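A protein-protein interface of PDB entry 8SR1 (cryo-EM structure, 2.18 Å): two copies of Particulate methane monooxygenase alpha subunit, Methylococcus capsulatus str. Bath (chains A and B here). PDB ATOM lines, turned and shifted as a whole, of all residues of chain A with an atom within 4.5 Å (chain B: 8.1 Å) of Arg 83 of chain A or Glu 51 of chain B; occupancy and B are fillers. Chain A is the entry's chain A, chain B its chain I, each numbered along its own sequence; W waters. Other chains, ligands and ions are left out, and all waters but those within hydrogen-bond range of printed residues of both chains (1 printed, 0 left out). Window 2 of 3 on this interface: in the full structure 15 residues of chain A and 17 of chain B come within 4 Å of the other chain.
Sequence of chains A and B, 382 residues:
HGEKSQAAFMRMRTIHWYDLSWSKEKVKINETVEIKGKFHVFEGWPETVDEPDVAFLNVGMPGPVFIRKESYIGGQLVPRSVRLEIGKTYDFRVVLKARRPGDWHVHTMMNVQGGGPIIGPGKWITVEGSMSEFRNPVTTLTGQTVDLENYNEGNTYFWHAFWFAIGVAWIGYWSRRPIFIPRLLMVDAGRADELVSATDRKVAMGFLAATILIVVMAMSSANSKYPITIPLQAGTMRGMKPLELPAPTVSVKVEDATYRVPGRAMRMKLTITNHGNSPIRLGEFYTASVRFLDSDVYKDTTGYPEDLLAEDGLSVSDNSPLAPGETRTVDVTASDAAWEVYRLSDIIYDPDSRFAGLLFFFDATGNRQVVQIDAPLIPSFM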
ATOM      1  N   PRO A  52     -16.715  -9.063 -29.936  1.00  0.00           N
ATOM      2  CA  PRO A  52     -16.266  -9.161 -28.540  1.00  0.00           C
ATOM      3  C   PRO A  52     -16.214 -10.594 -28.035  1.00  0.00           C
ATOM      4  O   PRO A  52     -16.753 -10.910 -26.971  1.00  0.00           O
ATOM      5  CB  PRO A  52     -17.310  -8.334 -27.781  1.00  0.00           C
ATOM      6  CG  PRO A  52     -18.529  -8.398 -28.629  1.00  0.00           C
ATOM      7  CD  PRO A  52     -18.052  -8.459 -30.050  1.00  0.00           C
ATOM      8  N   ASP A  53     -15.559 -11.470 -28.802  1.00  0.00           N
ATOM      9  CA  ASP A  53     -15.347 -12.842 -28.356  1.00  0.00           C
ATOM     10  C   ASP A  53     -14.430 -12.892 -27.144  1.00  0.00           C
ATOM     11  O   ASP A  53     -14.593 -13.759 -26.280  1.00  0.00           O
ATOM     12  CB  ASP A  53     -14.766 -13.678 -29.495  1.00  0.00           C
ATOM     13  CG  ASP A  53     -15.781 -13.964 -30.582  1.00  0.00           C
ATOM     14  OD1 ASP A  53     -16.974 -13.664 -30.380  1.00  0.00           O
ATOM     15  OD2 ASP A  53     -15.379 -14.490 -31.640  1.00  0.00           O
ATOM     16  N   VAL A  82     -13.444 -12.143 -20.864  1.00  0.00           N
ATOM     17  CA  VAL A  82     -14.740 -12.798 -20.972  1.00  0.00           C
ATOM     18  C   VAL A  82     -15.233 -12.703 -22.407  1.00  0.00           C
ATOM     19  O   VAL A  82     -14.760 -11.891 -23.205  1.00  0.00           O
ATOM     20  CB  VAL A  82     -15.779 -12.198 -20.006  1.00  0.00           C
ATOM     21  CG1 VAL A  82     -15.268 -12.251 -18.582  1.00  0.00           C
ATOM     22  CG2 VAL A  82     -16.118 -10.775 -20.404  1.00  0.00           C
ATOM     23  N   ARG A  83     -16.199 -13.553 -22.725  1.00  0.00           N
ATOM     24  CA  ARG A  83     -16.835 -13.563 -24.033  1.00  0.00           C
ATOM     25  C   ARG A  83     -18.196 -12.887 -23.934  1.00  0.00           C
ATOM     26  O   ARG A  83     -19.016 -13.254 -23.087  1.00  0.00           O
ATOM     27  CB  ARG A  83     -16.991 -14.990 -24.556  1.00  0.00           C
ATOM     28  CG  ARG A  83     -17.936 -15.109 -25.737  1.00  0.00           C
ATOM     29  CD  ARG A  83     -18.034 -16.544 -26.217  1.00  0.00           C
ATOM     30  NE  ARG A  83     -17.026 -16.842 -27.226  1.00  0.00           N
ATOM     31  CZ  ARG A  83     -17.259 -16.871 -28.531  1.00  0.00           C
ATOM     32  NH1 ARG A  83     -18.463 -16.628 -29.026  1.00  0.00           N
ATOM     33  NH2 ARG A  83     -16.259 -17.151 -29.361  1.00  0.00           N
ATOM     34  N   LEU A  84     -18.429 -11.906 -24.795  1.00  0.00           N
ATOM     35  CA  LEU A  84     -19.693 -11.195 -24.856  1.00  0.00           C
ATOM     36  C   LEU A  84     -20.379 -11.493 -26.182  1.00  0.00           C
ATOM     37  O   LEU A  84     -19.714 -11.749 -27.191  1.00  0.00           O
ATOM     38  CB  LEU A  84     -19.488  -9.688 -24.696  1.00  0.00           C
ATOM     39  CG  LEU A  84     -18.851  -9.247 -23.377  1.00  0.00           C
ATOM     40  CD1 LEU A  84     -18.559  -7.756 -23.394  1.00  0.00           C
ATOM     41  CD2 LEU A  84     -19.737  -9.614 -22.201  1.00  0.00           C
ATOM     42  N   GLU A  85     -21.705 -11.461 -26.176  1.00  0.00           N
ATOM     43  CA  GLU A  85     -22.502 -11.735 -27.362  1.00  0.00           C
ATOM     44  C   GLU A  85     -23.103 -10.440 -27.886  1.00  0.00           C
ATOM     45  O   GLU A  85     -23.636  -9.637 -27.113  1.00  0.00           O
ATOM     46  CB  GLU A  85     -23.602 -12.753 -27.061  1.00  0.00           C
ATOM     47  CG  GLU A  85     -23.098 -14.097 -26.541  1.00  0.00           C
ATOM     48  CD  GLU A  85     -22.036 -14.733 -27.426  1.00  0.00           C
ATOM     49  OE1 GLU A  85     -22.058 -14.512 -28.655  1.00  0.00           O
ATOM     50  OE2 GLU A  85     -21.176 -15.461 -26.886  1.00  0.00           O
ATOM     51  N   THR A 236      -9.771 -16.975 -21.245  1.00  0.00           N
ATOM     52  CA  THR A 236     -11.057 -16.314 -21.422  1.00  0.00           C
ATOM     53  C   THR A 236     -12.173 -17.149 -20.810  1.00  0.00           C
ATOM     54  O   THR A 236     -12.196 -18.377 -20.934  1.00  0.00           O
ATOM     55  CB  THR A 236     -11.330 -16.075 -22.911  1.00  0.00           C
ATOM     56  OG1 THR A 236     -10.275 -15.283 -23.467  1.00  0.00           O
ATOM     57  CG2 THR A 236     -12.653 -15.348 -23.108  1.00  0.00           C
ATOM     58  N   MET A 237     -13.099 -16.475 -20.137  1.00  0.00           N
ATOM     59  CA  MET A 237     -14.188 -17.131 -19.427  1.00  0.00           C
ATOM     60  C   MET A 237     -15.465 -17.004 -20.247  1.00  0.00           C
ATOM     61  O   MET A 237     -15.896 -15.892 -20.570  1.00  0.00           O
ATOM     62  CB  MET A 237     -14.367 -16.515 -18.042  1.00  0.00           C
ATOM     63  CG  MET A 237     -13.288 -16.929 -17.054  1.00  0.00           C
ATOM     64  SD  MET A 237     -13.320 -15.964 -15.535  1.00  0.00           S
ATOM     65  CE  MET A 237     -15.024 -16.176 -15.052  1.00  0.00           C
ATOM     66  N   ARG A 238     -16.065 -18.141 -20.582  1.00  0.00           N
ATOM     67  CA  ARG A 238     -17.287 -18.184 -21.365  1.00  0.00           C
ATOM     68  C   ARG A 238     -18.498 -18.217 -20.440  1.00  0.00           C
ATOM     69  O   ARG A 238     -18.385 -18.239 -19.213  1.00  0.00           O
ATOM     70  CB  ARG A 238     -17.283 -19.395 -22.298  1.00  0.00           C
ATOM     71  CG  ARG A 238     -17.004 -19.071 -23.751  1.00  0.00           C
ATOM     72  CD  ARG A 238     -16.544 -20.312 -24.494  1.00  0.00           C
ATOM     73  NE  ARG A 238     -16.586 -20.145 -25.942  1.00  0.00           N
ATOM     74  CZ  ARG A 238     -17.695 -20.167 -26.668  1.00  0.00           C
ATOM     75  NH1 ARG A 238     -18.881 -20.357 -26.113  1.00  0.00           N
ATOM     76  NH2 ARG A 238     -17.612 -19.998 -27.983  1.00  0.00           N
ATOM     77  N   MET A 240     -20.989 -15.947 -19.886  1.00  0.00           N
ATOM     78  CA  MET A 240     -21.449 -14.751 -19.190  1.00  0.00           C
ATOM     79  C   MET A 240     -22.967 -14.700 -19.285  1.00  0.00           C
ATOM     80  O   MET A 240     -23.530 -14.863 -20.370  1.00  0.00           O
ATOM     81  CB  MET A 240     -20.816 -13.495 -19.785  1.00  0.00           C
ATOM     82  CG  MET A 240     -19.298 -13.439 -19.707  1.00  0.00           C
ATOM     83  SD  MET A 240     -18.654 -13.334 -18.024  1.00  0.00           S
ATOM     84  CE  MET A 240     -18.295 -15.052 -17.663  1.00  0.00           C
ATOM     85  N   VAL B  41     -21.147 -31.015 -26.051  1.00  0.00           N
ATOM     86  CA  VAL B  41     -20.104 -30.005 -26.195  1.00  0.00           C
ATOM     87  C   VAL B  41     -20.299 -28.961 -25.105  1.00  0.00           C
ATOM     88  O   VAL B  41     -21.340 -28.298 -25.048  1.00  0.00           O
ATOM     89  CB  VAL B  41     -20.135 -29.370 -27.589  1.00  0.00           C
ATOM     90  CG1 VAL B  41     -18.913 -28.497 -27.800  1.00  0.00           C
ATOM     91  CG2 VAL B  41     -20.217 -30.448 -28.657  1.00  0.00           C
ATOM     92  N   GLU B  43     -20.416 -25.743 -22.814  1.00  0.00           N
ATOM     93  CA  GLU B  43     -20.601 -24.331 -23.134  1.00  0.00           C
ATOM     94  C   GLU B  43     -19.345 -23.521 -22.834  1.00  0.00           C
ATOM     95  O   GLU B  43     -18.979 -22.624 -23.604  1.00  0.00           O
ATOM     96  CB  GLU B  43     -21.794 -23.769 -22.364  1.00  0.00           C
ATOM     97  CG  GLU B  43     -23.141 -24.202 -22.912  1.00  0.00           C
ATOM     98  CD  GLU B  43     -23.582 -25.550 -22.375  1.00  0.00           C
ATOM     99  OE1 GLU B  43     -22.807 -26.171 -21.620  1.00  0.00           O
ATOM    100  OE2 GLU B  43     -24.702 -25.988 -22.711  1.00  0.00           O
ATOM    101  N   TRP B  45     -16.329 -23.745 -23.411  1.00  0.00           N
ATOM    102  CA  TRP B  45     -15.241 -24.269 -24.222  1.00  0.00           C
ATOM    103  C   TRP B  45     -13.987 -23.421 -24.017  1.00  0.00           C
ATOM    104  O   TRP B  45     -14.046 -22.191 -24.163  1.00  0.00           O
ATOM    105  CB  TRP B  45     -15.660 -24.253 -25.690  1.00  0.00           C
ATOM    106  CG  TRP B  45     -14.764 -24.982 -26.630  1.00  0.00           C
ATOM    107  CD1 TRP B  45     -13.760 -24.450 -27.382  1.00  0.00           C
ATOM    108  CD2 TRP B  45     -14.825 -26.370 -26.970  1.00  0.00           C
ATOM    109  NE1 TRP B  45     -13.173 -25.424 -28.147  1.00  0.00           N
ATOM    110  CE2 TRP B  45     -13.812 -26.614 -27.914  1.00  0.00           C
ATOM    111  CE3 TRP B  45     -15.631 -27.434 -26.559  1.00  0.00           C
ATOM    112  CZ2 TRP B  45     -13.582 -27.877 -28.454  1.00  0.00           C
ATOM    113  CZ3 TRP B  45     -15.402 -28.685 -27.099  1.00  0.00           C
ATOM    114  CH2 TRP B  45     -14.386 -28.896 -28.031  1.00  0.00           C
ATOM    115  N   PRO B  46     -12.851 -24.024 -23.673  1.00  0.00           N
ATOM    116  CA  PRO B  46     -11.652 -23.226 -23.383  1.00  0.00           C
ATOM    117  C   PRO B  46     -11.211 -22.425 -24.598  1.00  0.00           C
ATOM    118  O   PRO B  46     -11.266 -22.904 -25.734  1.00  0.00           O
ATOM    119  CB  PRO B  46     -10.612 -24.280 -22.985  1.00  0.00           C
ATOM    120  CG  PRO B  46     -11.105 -25.553 -23.577  1.00  0.00           C
ATOM    121  CD  PRO B  46     -12.597 -25.471 -23.582  1.00  0.00           C
ATOM    122  N   GLU B  47     -10.767 -21.192 -24.348  1.00  0.00           N
ATOM    123  CA  GLU B  47     -10.351 -20.316 -25.439  1.00  0.00           C
ATOM    124  C   GLU B  47      -9.109 -20.832 -26.150  1.00  0.00           C
ATOM    125  O   GLU B  47      -8.903 -20.515 -27.327  1.00  0.00           O
ATOM    126  CB  GLU B  47     -10.105 -18.902 -24.913  1.00  0.00           C
ATOM    127  CG  GLU B  47      -8.793 -18.729 -24.163  1.00  0.00           C
ATOM    128  CD  GLU B  47      -8.185 -17.355 -24.369  1.00  0.00           C
ATOM    129  OE1 GLU B  47      -8.371 -16.780 -25.459  1.00  0.00           O
ATOM    130  OE2 GLU B  47      -7.524 -16.851 -23.437  1.00  0.00           O
ATOM    131  N   THR B  48      -8.283 -21.625 -25.466  1.00  0.00           N
ATOM    132  CA  THR B  48      -7.092 -22.180 -26.090  1.00  0.00           C
ATOM    133  C   THR B  48      -7.424 -23.250 -27.118  1.00  0.00           C
ATOM    134  O   THR B  48      -6.594 -23.538 -27.988  1.00  0.00           O
ATOM    135  CB  THR B  48      -6.168 -22.753 -25.019  1.00  0.00           C
ATOM    136  OG1 THR B  48      -5.018 -23.341 -25.639  1.00  0.00           O
ATOM    137  CG2 THR B  48      -6.904 -23.807 -24.205  1.00  0.00           C
ATOM    138  N   VAL B  49      -8.606 -23.841 -27.037  1.00  0.00           N
ATOM    139  CA  VAL B  49      -9.082 -24.789 -28.035  1.00  0.00           C
ATOM    140  C   VAL B  49      -9.971 -24.047 -29.012  1.00  0.00           C
ATOM    141  O   VAL B  49     -10.913 -23.350 -28.620  1.00  0.00           O
ATOM    142  CB  VAL B  49      -9.840 -25.966 -27.384  1.00  0.00           C
ATOM    143  CG1 VAL B  49     -10.259 -26.969 -28.436  1.00  0.00           C
ATOM    144  CG2 VAL B  49      -8.980 -26.627 -26.344  1.00  0.00           C
ATOM    145  N   ASP B  50      -9.669 -24.187 -30.298  1.00  0.00           N
ATOM    146  CA  ASP B  50     -10.525 -23.600 -31.314  1.00  0.00           C
ATOM    147  C   ASP B  50     -11.918 -24.209 -31.232  1.00  0.00           C
ATOM    148  O   ASP B  50     -12.097 -25.369 -30.852  1.00  0.00           O
ATOM    149  CB  ASP B  50      -9.941 -23.813 -32.711  1.00  0.00           C
ATOM    150  CG  ASP B  50      -8.861 -22.806 -33.053  1.00  0.00           C
ATOM    151  OD1 ASP B  50      -8.344 -22.141 -32.130  1.00  0.00           O
ATOM    152  OD2 ASP B  50      -8.528 -22.676 -34.249  1.00  0.00           O
ATOM    153  N   GLU B  51     -12.915 -23.398 -31.570  1.00  0.00           N
ATOM    154  CA  GLU B  51     -14.286 -23.863 -31.538  1.00  0.00           C
ATOM    155  C   GLU B  51     -14.453 -25.052 -32.484  1.00  0.00           C
ATOM    156  O   GLU B  51     -13.825 -25.104 -33.543  1.00  0.00           O
ATOM    157  CB  GLU B  51     -15.239 -22.740 -31.931  1.00  0.00           C
ATOM    158  CG  GLU B  51     -15.773 -21.958 -30.746  1.00  0.00           C
ATOM    159  CD  GLU B  51     -16.093 -20.519 -31.085  1.00  0.00           C
ATOM    160  OE1 GLU B  51     -15.154 -19.753 -31.375  1.00  0.00           O
ATOM    161  OE2 GLU B  51     -17.287 -20.155 -31.057  1.00  0.00           O
ATOM    162  N   PRO B  52     -15.291 -26.025 -32.121  1.00  0.00           N
ATOM    163  CA  PRO B  52     -15.397 -27.236 -32.945  1.00  0.00           C
ATOM    164  C   PRO B  52     -16.124 -26.996 -34.260  1.00  0.00           C
ATOM    165  O   PRO B  52     -17.054 -27.725 -34.611  1.00  0.00           O
ATOM    166  CB  PRO B  52     -16.175 -28.201 -32.042  1.00  0.00           C
ATOM    167  CG  PRO B  52     -16.963 -27.321 -31.142  1.00  0.00           C
ATOM    168  CD  PRO B  52     -16.131 -26.093 -30.915  1.00  0.00           C
ATOM    169  N   ASP B  53     -15.695 -25.964 -34.994  1.00  0.00           N
ATOM    170  CA  ASP B  53     -16.239 -25.717 -36.323  1.00  0.00           C
ATOM    171  C   ASP B  53     -15.872 -26.834 -37.287  1.00  0.00           C
ATOM    172  O   ASP B  53     -16.655 -27.158 -38.186  1.00  0.00           O
ATOM    173  CB  ASP B  53     -15.739 -24.373 -36.851  1.00  0.00           C
ATOM    174  CG  ASP B  53     -16.372 -23.196 -36.138  1.00  0.00           C
ATOM    175  OD1 ASP B  53     -17.320 -23.409 -35.358  1.00  0.00           O
ATOM    176  OD2 ASP B  53     -15.915 -22.057 -36.366  1.00  0.00           O
ATOM    177  N   VAL B  54     -14.688 -27.415 -37.131  1.00  0.00           N
ATOM    178  CA  VAL B  54     -14.239 -28.538 -37.944  1.00  0.00           C
ATOM    179  C   VAL B  54     -13.801 -29.625 -36.971  1.00  0.00           C
ATOM    180  O   VAL B  54     -12.770 -29.490 -36.301  1.00  0.00           O
ATOM    181  CB  VAL B  54     -13.101 -28.155 -38.897  1.00  0.00           C
ATOM    182  CG1 VAL B  54     -12.699 -29.345 -39.731  1.00  0.00           C
ATOM    183  CG2 VAL B  54     -13.518 -26.995 -39.790  1.00  0.00           C
ATOM    184  N   ALA B  55     -14.582 -30.696 -36.880  1.00  0.00           N
ATOM    185  CA  ALA B  55     -14.306 -31.790 -35.962  1.00  0.00           C
ATOM    186  C   ALA B  55     -14.476 -33.118 -36.681  1.00  0.00           C
ATOM    187  O   ALA B  55     -15.281 -33.244 -37.605  1.00  0.00           O
ATOM    188  CB  ALA B  55     -15.221 -31.738 -34.732  1.00  0.00           C
ATOM    189  N   VAL B  82     -16.728 -32.763 -39.538  1.00  0.00           N
ATOM    190  CA  VAL B  82     -18.067 -32.241 -39.323  1.00  0.00           C
ATOM    191  C   VAL B  82     -17.987 -30.989 -38.463  1.00  0.00           C
ATOM    192  O   VAL B  82     -16.987 -30.723 -37.793  1.00  0.00           O
ATOM    193  CB  VAL B  82     -19.003 -33.277 -38.673  1.00  0.00           C
ATOM    194  CG1 VAL B  82     -19.048 -34.542 -39.504  1.00  0.00           C
ATOM    195  CG2 VAL B  82     -18.559 -33.581 -37.254  1.00  0.00           C
ATOM    196  N   ARG B  83     -19.065 -30.216 -38.493  1.00  0.00           N
ATOM    197  CA  ARG B  83     -19.189 -29.013 -37.687  1.00  0.00           C
ATOM    198  C   ARG B  83     -20.087 -29.301 -36.493  1.00  0.00           C
ATOM    199  O   ARG B  83     -21.209 -29.792 -36.656  1.00  0.00           O
ATOM    200  CB  ARG B  83     -19.759 -27.857 -38.509  1.00  0.00           C
ATOM    201  CG  ARG B  83     -20.233 -26.684 -37.673  1.00  0.00           C
ATOM    202  CD  ARG B  83     -20.771 -25.569 -38.548  1.00  0.00           C
ATOM    203  NE  ARG B  83     -19.721 -24.636 -38.932  1.00  0.00           N
ATOM    204  CZ  ARG B  83     -19.512 -23.462 -38.352  1.00  0.00           C
ATOM    205  NH1 ARG B  83     -20.272 -23.038 -37.354  1.00  0.00           N
ATOM    206  NH2 ARG B  83     -18.519 -22.693 -38.786  1.00  0.00           N
ATOM    207  N   LEU B  84     -19.592 -28.998 -35.299  1.00  0.00           N
ATOM    208  CA  LEU B  84     -20.342 -29.171 -34.069  1.00  0.00           C
ATOM    209  C   LEU B  84     -20.626 -27.809 -33.450  1.00  0.00           C
ATOM    210  O   LEU B  84     -19.849 -26.865 -33.625  1.00  0.00           O
ATOM    211  CB  LEU B  84     -19.579 -30.053 -33.077  1.00  0.00           C
ATOM    212  CG  LEU B  84     -19.275 -31.472 -33.556  1.00  0.00           C
ATOM    213  CD1 LEU B  84     -18.390 -32.198 -32.557  1.00  0.00           C
ATOM    214  CD2 LEU B  84     -20.558 -32.244 -33.807  1.00  0.00           C
ATOM    215  N   GLU B  85     -21.737 -27.712 -32.733  1.00  0.00           N
ATOM    216  CA  GLU B  85     -22.150 -26.473 -32.090  1.00  0.00           C
ATOM    217  C   GLU B  85     -21.942 -26.582 -30.589  1.00  0.00           C
ATOM    218  O   GLU B  85     -22.301 -27.593 -29.976  1.00  0.00           O
ATOM    219  CB  GLU B  85     -23.609 -26.149 -32.408  1.00  0.00           C
ATOM    220  CG  GLU B  85     -23.920 -26.005 -33.895  1.00  0.00           C
ATOM    221  CD  GLU B  85     -23.007 -25.023 -34.615  1.00  0.00           C
ATOM    222  OE1 GLU B  85     -22.539 -24.053 -33.982  1.00  0.00           O
ATOM    223  OE2 GLU B  85     -22.759 -25.223 -35.824  1.00  0.00           O
ATOM    224  N   ILE B  86     -21.354 -25.541 -30.002  1.00  0.00           N
ATOM    225  CA  ILE B  86     -21.093 -25.519 -28.568  1.00  0.00           C
ATOM    226  C   ILE B  86     -22.413 -25.502 -27.813  1.00  0.00           C
ATOM    227  O   ILE B  86     -23.327 -24.733 -28.139  1.00  0.00           O
ATOM    228  CB  ILE B  86     -20.222 -24.309 -28.207  1.00  0.00           C
ATOM    229  CG1 ILE B  86     -18.800 -24.508 -28.724  1.00  0.00           C
ATOM    230  CG2 ILE B  86     -20.209 -24.077 -26.710  1.00  0.00           C
ATOM    231  CD1 ILE B  86     -17.865 -23.404 -28.328  1.00  0.00           C
ATOM    232  N   VAL B 112     -10.515 -32.014 -32.877  1.00  0.00           N
ATOM    233  CA  VAL B 112     -10.966 -30.668 -33.210  1.00  0.00           C
ATOM    234  C   VAL B 112      -9.859 -29.969 -33.985  1.00  0.00           C
ATOM    235  O   VAL B 112      -8.676 -30.088 -33.642  1.00  0.00           O
ATOM    236  CB  VAL B 112     -11.354 -29.882 -31.945  1.00  0.00           C
ATOM    237  CG1 VAL B 112     -11.779 -28.469 -32.299  1.00  0.00           C
ATOM    238  CG2 VAL B 112     -12.472 -30.598 -31.217  1.00  0.00           C
ATOM    239  N   GLN B 113     -10.249 -29.247 -35.039  1.00  0.00           N
ATOM    240  CA  GLN B 113      -9.292 -28.682 -35.988  1.00  0.00           C
ATOM    241  C   GLN B 113      -8.183 -27.885 -35.312  1.00  0.00           C
ATOM    242  O   GLN B 113      -7.006 -28.042 -35.643  1.00  0.00           O
ATOM    243  CB  GLN B 113     -10.033 -27.803 -36.998  1.00  0.00           C
ATOM    244  CG  GLN B 113      -9.128 -26.916 -37.839  1.00  0.00           C
ATOM    245  CD  GLN B 113      -8.658 -27.590 -39.107  1.00  0.00           C
ATOM    246  OE1 GLN B 113      -7.670 -28.322 -39.104  1.00  0.00           O
ATOM    247  NE2 GLN B 113      -9.363 -27.345 -40.203  1.00  0.00           N
ATOM    248  N   GLY B 114      -8.534 -27.031 -34.358  1.00  0.00           N
ATOM    249  CA  GLY B 114      -7.517 -26.210 -33.732  1.00  0.00           C
ATOM    250  C   GLY B 114      -7.321 -26.459 -32.252  1.00  0.00           C
ATOM    251  O   GLY B 114      -6.860 -25.570 -31.530  1.00  0.00           O
ATOM    252  N   GLY B 115      -7.674 -27.649 -31.776  1.00  0.00           N
ATOM    253  CA  GLY B 115      -7.471 -27.941 -30.373  1.00  0.00           C
ATOM    254  C   GLY B 115      -6.843 -29.281 -30.060  1.00  0.00           C
ATOM    255  O   GLY B 115      -6.379 -29.494 -28.939  1.00  0.00           O
HETATM  256  O   HOH W   1     -10.890 -20.786 -21.262  1.00  0.00           O
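NH2 of Arg 83 of chain A is in salt-bridge range of OE1 of Glu 51 of chain B (3.5 Å). OG1 of Thr 236 of chain A sits close to OE1 of Glu 47 of chain B. NH1 of Arg 238 of chain A is in hydrogen-bond range of O of Glu 43 of chain B, at 3.4 Å. NH2 of Arg 238 of chain A is in salt-bridge range of OE2 of Glu 51 of chain B (3.1 Å).
The side-chain carboxylate (OD1) of Asp 53 of chain A lies within salt-bridge range of the guanidinium group (NH1) of Arg 83 of chain A, at 3.6 Å. The side-chain carboxylate (OE2) of Glu 85 of chain A lies within salt-bridge range of the guanidinium group (NH1) of Arg 83 of chain A (3.6 Å). The backbone NH of Arg 83 of chain A sits at hydrogen-bond distance from the backbone carbonyl oxygen of Met 237 of chain A (3.2 Å). The indole nitrogen (NE1) of Trp 45 of chain B is in hydrogen-bond range of the backbone carbonyl oxygen (O) of Val 49 of chain B (3.1 Å). The indole nitrogen (NE1) of Trp 45 of chain B sits at hydrogen-bond distance from the backbone carbonyl oxygen (O) of Asp 50 of chain B (2.9 Å).
Among the printed residues, pairs that only touch across the chains: Arg 238 of chain A with Trp 45 of chain B (3.1 Å) and Arg 238 of chain A with Ile 86 of chain B (3.4 Å).
Asp 53 of chain A touches none of the printed residues of chain B. Of chain B, only Glu 51 (3.5 Å) comes within 4 Å of Arg 83 of chain A. Of the printed residues of chain B, Arg 238 of chain A touches Glu 43 (3.4 Å), Trp 45 (3.1 Å), Glu 51 (3.1 Å) and Ile 86 (3.4 Å). Of the printed residues of chain A, Glu 43 of chain B touches Arg 238 (3.4 Å). Of the printed residues of chain A, Trp 45 of chain B touches Arg 238. Glu 51 of chain B touches just these residues of chain A: Arg 83 (3.5 Å) and Arg 238 (3.1 Å). The nearest residue of chain B that does not touch Arg 83 of chain A is Ile 86 of chain B (6.5 Å). The nearest printed residue of chain B that does not touch Thr 236 of chain A is Trp 45 of chain B (5.3 Å).
Of the 22 printed residues of chain B, 5 touch a printed residue of chain A.
Positions printed for both chains: 52, 53, 82, 83, 84 and 85.
Water W1 lies within hydrogen-bond range of O of Thr 236 of chain A (2.8 Å) and N of Glu 47 of chain B (3.1 Å).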
